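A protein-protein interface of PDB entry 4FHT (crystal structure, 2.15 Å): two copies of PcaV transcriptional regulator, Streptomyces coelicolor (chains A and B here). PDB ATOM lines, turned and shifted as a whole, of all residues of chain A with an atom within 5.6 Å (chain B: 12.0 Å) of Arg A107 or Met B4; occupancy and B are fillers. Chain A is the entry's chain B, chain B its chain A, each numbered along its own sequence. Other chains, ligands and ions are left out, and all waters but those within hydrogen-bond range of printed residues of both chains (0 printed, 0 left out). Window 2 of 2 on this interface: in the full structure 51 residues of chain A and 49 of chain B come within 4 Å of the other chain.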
ATOM      1  N   VAL A  48     -14.456  -4.484  -1.405  1.00  0.00           N
ATOM      2  CA  VAL A  48     -14.222  -5.009  -2.745  1.00  0.00           C
ATOM      3  C   VAL A  48     -14.933  -4.128  -3.765  1.00  0.00           C
ATOM      4  O   VAL A  48     -14.388  -3.819  -4.829  1.00  0.00           O
ATOM      5  CB  VAL A  48     -14.717  -6.463  -2.879  1.00  0.00           C
ATOM      6  CG1 VAL A  48     -14.626  -6.932  -4.322  1.00  0.00           C
ATOM      7  CG2 VAL A  48     -13.919  -7.380  -1.969  1.00  0.00           C
ATOM      8  N   GLY A 102      -7.471 -10.716   2.922  1.00  0.00           N
ATOM      9  CA  GLY A 102      -8.856 -10.283   2.985  1.00  0.00           C
ATOM     10  C   GLY A 102      -9.620 -10.615   1.718  1.00  0.00           C
ATOM     11  O   GLY A 102     -10.725 -11.155   1.775  1.00  0.00           O
ATOM     12  N   LEU A 103      -9.026 -10.295   0.573  1.00  0.00           N
ATOM     13  CA  LEU A 103      -9.640 -10.597  -0.718  1.00  0.00           C
ATOM     14  C   LEU A 103      -9.739 -12.105  -0.938  1.00  0.00           C
ATOM     15  O   LEU A 103     -10.707 -12.597  -1.519  1.00  0.00           O
ATOM     16  CB  LEU A 103      -8.847  -9.947  -1.856  1.00  0.00           C
ATOM     17  CG  LEU A 103      -9.368 -10.213  -3.272  1.00  0.00           C
ATOM     18  CD1 LEU A 103     -10.823  -9.784  -3.399  1.00  0.00           C
ATOM     19  CD2 LEU A 103      -8.504  -9.508  -4.310  1.00  0.00           C
ATOM     20  N   ARG A 104      -8.734 -12.835  -0.465  1.00  0.00           N
ATOM     21  CA  ARG A 104      -8.725 -14.288  -0.575  1.00  0.00           C
ATOM     22  C   ARG A 104      -9.860 -14.897   0.246  1.00  0.00           C
ATOM     23  O   ARG A 104     -10.535 -15.825  -0.201  1.00  0.00           O
ATOM     24  CB  ARG A 104      -7.379 -14.849  -0.119  1.00  0.00           C
ATOM     25  CG  ARG A 104      -7.271 -16.361  -0.201  1.00  0.00           C
ATOM     26  CD  ARG A 104      -5.964 -16.845   0.409  1.00  0.00           C
ATOM     27  NE  ARG A 104      -5.931 -18.296   0.567  1.00  0.00           N
ATOM     28  CZ  ARG A 104      -6.443 -18.947   1.609  1.00  0.00           C
ATOM     29  NH1 ARG A 104      -7.035 -18.276   2.588  1.00  0.00           N
ATOM     30  NH2 ARG A 104      -6.366 -20.269   1.669  1.00  0.00           N
ATOM     31  N   VAL A 105     -10.062 -14.367   1.447  1.00  0.00           N
ATOM     32  CA  VAL A 105     -11.151 -14.819   2.302  1.00  0.00           C
ATOM     33  C   VAL A 105     -12.495 -14.458   1.682  1.00  0.00           C
ATOM     34  O   VAL A 105     -13.420 -15.271   1.670  1.00  0.00           O
ATOM     35  CB  VAL A 105     -11.054 -14.216   3.719  1.00  0.00           C
ATOM     36  CG1 VAL A 105     -12.328 -14.480   4.504  1.00  0.00           C
ATOM     37  CG2 VAL A 105      -9.851 -14.785   4.453  1.00  0.00           C
ATOM     38  N   HIS A 106     -12.592 -13.239   1.158  1.00  0.00           N
ATOM     39  CA  HIS A 106     -13.820 -12.779   0.518  1.00  0.00           C
ATOM     40  C   HIS A 106     -14.218 -13.698  -0.631  1.00  0.00           C
ATOM     41  O   HIS A 106     -15.364 -14.144  -0.713  1.00  0.00           O
ATOM     42  CB  HIS A 106     -13.665 -11.346   0.007  1.00  0.00           C
ATOM     43  CG  HIS A 106     -14.845 -10.856  -0.774  1.00  0.00           C
ATOM     44  ND1 HIS A 106     -14.918 -10.945  -2.148  1.00  0.00           N
ATOM     45  CD2 HIS A 106     -16.005 -10.282  -0.374  1.00  0.00           C
ATOM     46  CE1 HIS A 106     -16.067 -10.441  -2.560  1.00  0.00           C
ATOM     47  NE2 HIS A 106     -16.746 -10.032  -1.503  1.00  0.00           N
ATOM     48  N   ARG A 107     -13.263 -13.988  -1.508  1.00  0.00           N
ATOM     49  CA  ARG A 107     -13.524 -14.847  -2.657  1.00  0.00           C
ATOM     50  C   ARG A 107     -13.929 -16.260  -2.244  1.00  0.00           C
ATOM     51  O   ARG A 107     -14.875 -16.824  -2.792  1.00  0.00           O
ATOM     52  CB  ARG A 107     -12.313 -14.893  -3.589  1.00  0.00           C
ATOM     53  CG  ARG A 107     -12.406 -15.967  -4.660  1.00  0.00           C
ATOM     54  CD  ARG A 107     -11.569 -15.611  -5.875  1.00  0.00           C
ATOM     55  NE  ARG A 107     -12.171 -14.530  -6.650  1.00  0.00           N
ATOM     56  CZ  ARG A 107     -11.582 -13.926  -7.678  1.00  0.00           C
ATOM     57  NH1 ARG A 107     -10.365 -14.287  -8.059  1.00  0.00           N
ATOM     58  NH2 ARG A 107     -12.210 -12.955  -8.325  1.00  0.00           N
ATOM     59  N   ARG A 108     -13.214 -16.823  -1.277  1.00  0.00           N
ATOM     60  CA  ARG A 108     -13.463 -18.193  -0.846  1.00  0.00           C
ATOM     61  C   ARG A 108     -14.860 -18.373  -0.250  1.00  0.00           C
ATOM     62  O   ARG A 108     -15.569 -19.326  -0.580  1.00  0.00           O
ATOM     63  CB  ARG A 108     -12.394 -18.641   0.152  1.00  0.00           C
ATOM     64  CG  ARG A 108     -12.516 -20.096   0.574  1.00  0.00           C
ATOM     65  CD  ARG A 108     -11.283 -20.556   1.336  1.00  0.00           C
ATOM     66  NE  ARG A 108     -11.002 -19.703   2.486  1.00  0.00           N
ATOM     67  CZ  ARG A 108     -11.548 -19.863   3.688  1.00  0.00           C
ATOM     68  NH1 ARG A 108     -12.411 -20.848   3.902  1.00  0.00           N
ATOM     69  NH2 ARG A 108     -11.232 -19.036   4.676  1.00  0.00           N
ATOM     70  N   LEU A 109     -15.257 -17.452   0.621  1.00  0.00           N
ATOM     71  CA  LEU A 109     -16.568 -17.525   1.258  1.00  0.00           C
ATOM     72  C   LEU A 109     -17.711 -17.347   0.264  1.00  0.00           C
ATOM     73  O   LEU A 109     -18.765 -17.961   0.413  1.00  0.00           O
ATOM     74  CB  LEU A 109     -16.681 -16.498   2.386  1.00  0.00           C
ATOM     75  CG  LEU A 109     -15.739 -16.722   3.570  1.00  0.00           C
ATOM     76  CD1 LEU A 109     -16.049 -15.751   4.700  1.00  0.00           C
ATOM     77  CD2 LEU A 109     -15.827 -18.158   4.051  1.00  0.00           C
ATOM     78  N   GLY A 110     -17.491 -16.516  -0.751  1.00  0.00           N
ATOM     79  CA  GLY A 110     -18.504 -16.246  -1.758  1.00  0.00           C
ATOM     80  C   GLY A 110     -19.040 -17.501  -2.417  1.00  0.00           C
ATOM     81  O   GLY A 110     -20.242 -17.624  -2.660  1.00  0.00           O
ATOM     82  N   VAL A 111     -18.143 -18.440  -2.706  1.00  0.00           N
ATOM     83  CA  VAL A 111     -18.532 -19.721  -3.283  1.00  0.00           C
ATOM     84  C   VAL A 111     -19.454 -20.470  -2.326  1.00  0.00           C
ATOM     85  O   VAL A 111     -20.480 -21.022  -2.731  1.00  0.00           O
ATOM     86  CB  VAL A 111     -17.299 -20.593  -3.591  1.00  0.00           C
ATOM     87  CG1 VAL A 111     -17.730 -21.973  -4.066  1.00  0.00           C
ATOM     88  CG2 VAL A 111     -16.414 -19.914  -4.624  1.00  0.00           C
ATOM     89  N   MET B   4     -12.103  -9.813  -6.678  1.00  0.00           N
ATOM     90  CA  MET B   4     -12.262  -9.028  -7.898  1.00  0.00           C
ATOM     91  C   MET B   4     -13.677  -8.475  -8.027  1.00  0.00           C
ATOM     92  O   MET B   4     -13.869  -7.293  -8.314  1.00  0.00           O
ATOM     93  CB  MET B   4     -11.925  -9.876  -9.126  1.00  0.00           C
ATOM     94  CG  MET B   4     -12.136  -9.169 -10.454  1.00  0.00           C
ATOM     95  SD  MET B   4     -12.044 -10.302 -11.853  1.00  0.00           S
ATOM     96  CE  MET B   4     -10.445 -11.060 -11.573  1.00  0.00           C
ATOM     97  N   ALA B   5     -14.666  -9.337  -7.813  1.00  0.00           N
ATOM     98  CA  ALA B   5     -16.061  -8.952  -7.980  1.00  0.00           C
ATOM     99  C   ALA B   5     -16.826  -8.978  -6.663  1.00  0.00           C
ATOM    100  O   ALA B   5     -16.840  -9.988  -5.960  1.00  0.00           O
ATOM    101  CB  ALA B   5     -16.738  -9.855  -9.002  1.00  0.00           C
ATOM    102  N   ALA B   6     -17.466  -7.858  -6.337  1.00  0.00           N
ATOM    103  CA  ALA B   6     -18.304  -7.768  -5.150  1.00  0.00           C
ATOM    104  C   ALA B   6     -19.727  -8.219  -5.467  1.00  0.00           C
ATOM    105  O   ALA B   6     -20.176  -8.139  -6.611  1.00  0.00           O
ATOM    106  CB  ALA B   6     -18.307  -6.349  -4.609  1.00  0.00           C
ATOM    107  N   VAL B   7     -20.435  -8.692  -4.449  1.00  0.00           N
ATOM    108  CA  VAL B   7     -21.812  -9.126  -4.630  1.00  0.00           C
ATOM    109  C   VAL B   7     -22.781  -8.042  -4.175  1.00  0.00           C
ATOM    110  O   VAL B   7     -22.422  -7.161  -3.391  1.00  0.00           O
ATOM    111  CB  VAL B   7     -22.106 -10.432  -3.864  1.00  0.00           C
ATOM    112  CG1 VAL B   7     -21.246 -11.569  -4.399  1.00  0.00           C
ATOM    113  CG2 VAL B   7     -21.881 -10.239  -2.370  1.00  0.00           C
ATOM    114  N   ASP B   8     -24.008  -8.105  -4.679  1.00  0.00           N
ATOM    115  CA  ASP B   8     -25.051  -7.181  -4.259  1.00  0.00           C
ATOM    116  C   ASP B   8     -25.773  -7.755  -3.043  1.00  0.00           C
ATOM    117  O   ASP B   8     -26.529  -8.718  -3.159  1.00  0.00           O
ATOM    118  CB  ASP B   8     -26.034  -6.925  -5.406  1.00  0.00           C
ATOM    119  CG  ASP B   8     -27.099  -5.906  -5.049  1.00  0.00           C
ATOM    120  OD1 ASP B   8     -26.874  -5.102  -4.120  1.00  0.00           O
ATOM    121  OD2 ASP B   8     -28.163  -5.904  -5.703  1.00  0.00           O
ATOM    122  N   LEU B   9     -25.532  -7.156  -1.880  1.00  0.00           N
ATOM    123  CA  LEU B   9     -26.082  -7.659  -0.623  1.00  0.00           C
ATOM    124  C   LEU B   9     -27.604  -7.592  -0.560  1.00  0.00           C
ATOM    125  O   LEU B   9     -28.221  -8.239   0.284  1.00  0.00           O
ATOM    126  CB  LEU B   9     -25.480  -6.912   0.571  1.00  0.00           C
ATOM    127  CG  LEU B   9     -23.985  -7.115   0.822  1.00  0.00           C
ATOM    128  CD1 LEU B   9     -23.571  -6.487   2.141  1.00  0.00           C
ATOM    129  CD2 LEU B   9     -23.629  -8.594   0.789  1.00  0.00           C
ATOM    130  N   HIS B  12     -29.060 -10.953  -0.922  1.00  0.00           N
ATOM    131  CA  HIS B  12     -28.618 -11.954   0.047  1.00  0.00           C
ATOM    132  C   HIS B  12     -29.569 -12.030   1.235  1.00  0.00           C
ATOM    133  O   HIS B  12     -29.627 -11.104   2.041  1.00  0.00           O
ATOM    134  CB  HIS B  12     -27.197 -11.645   0.529  1.00  0.00           C
ATOM    135  CG  HIS B  12     -26.134 -12.003  -0.462  1.00  0.00           C
ATOM    136  ND1 HIS B  12     -25.015 -12.730  -0.120  1.00  0.00           N
ATOM    137  CD2 HIS B  12     -26.028 -11.748  -1.788  1.00  0.00           C
ATOM    138  CE1 HIS B  12     -24.261 -12.903  -1.191  1.00  0.00           C
ATOM    139  NE2 HIS B  12     -24.852 -12.316  -2.216  1.00  0.00           N
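Of the printed residues of chain B, Arg A107 touches Met B4 (3.2 Å). Met B4 touches just these residues of chain A: Leu A103 (3.5 Å) and Arg A107 (3.2 Å). Val A48 touches just these residues of chain B: Ala B5 and Ala B6. Leu A103 touches just one residue of chain B: Met B4. No residue of chain B comes within 4 Å of Val A105. Of chain B, only Ala B5 comes within 4 Å of His A106. No residue of chain B comes within 4 Å of Leu A109. No residue of chain B comes within 4 Å of Gly A110. No residue of chain B comes within 4 Å of Val A111. Of the printed residues of chain A, Ala B5 touches Val A48 (3.8 Å) and His A106 (3.5 Å). Of the printed residues of chain A, Ala B6 touches Val A48. Asp B8 touches none of the printed residues of chain A. Val B7 touches none of the printed residues of chain A. The nearest printed residue of chain A that does not touch Ala B6 is His A106 (4.3 Å).
Among the printed residues, pairs that only touch across the chains: Val A48 with Ala B5, Val A48 with Ala B6, Leu A103 with Met B4, His A106 with Ala B5 and Arg A107 with Met B4.
No position is printed for both chains. Of the 5 pairs that touch across the chains among the printed residues, none has its exchanged pair printed and touching as well.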
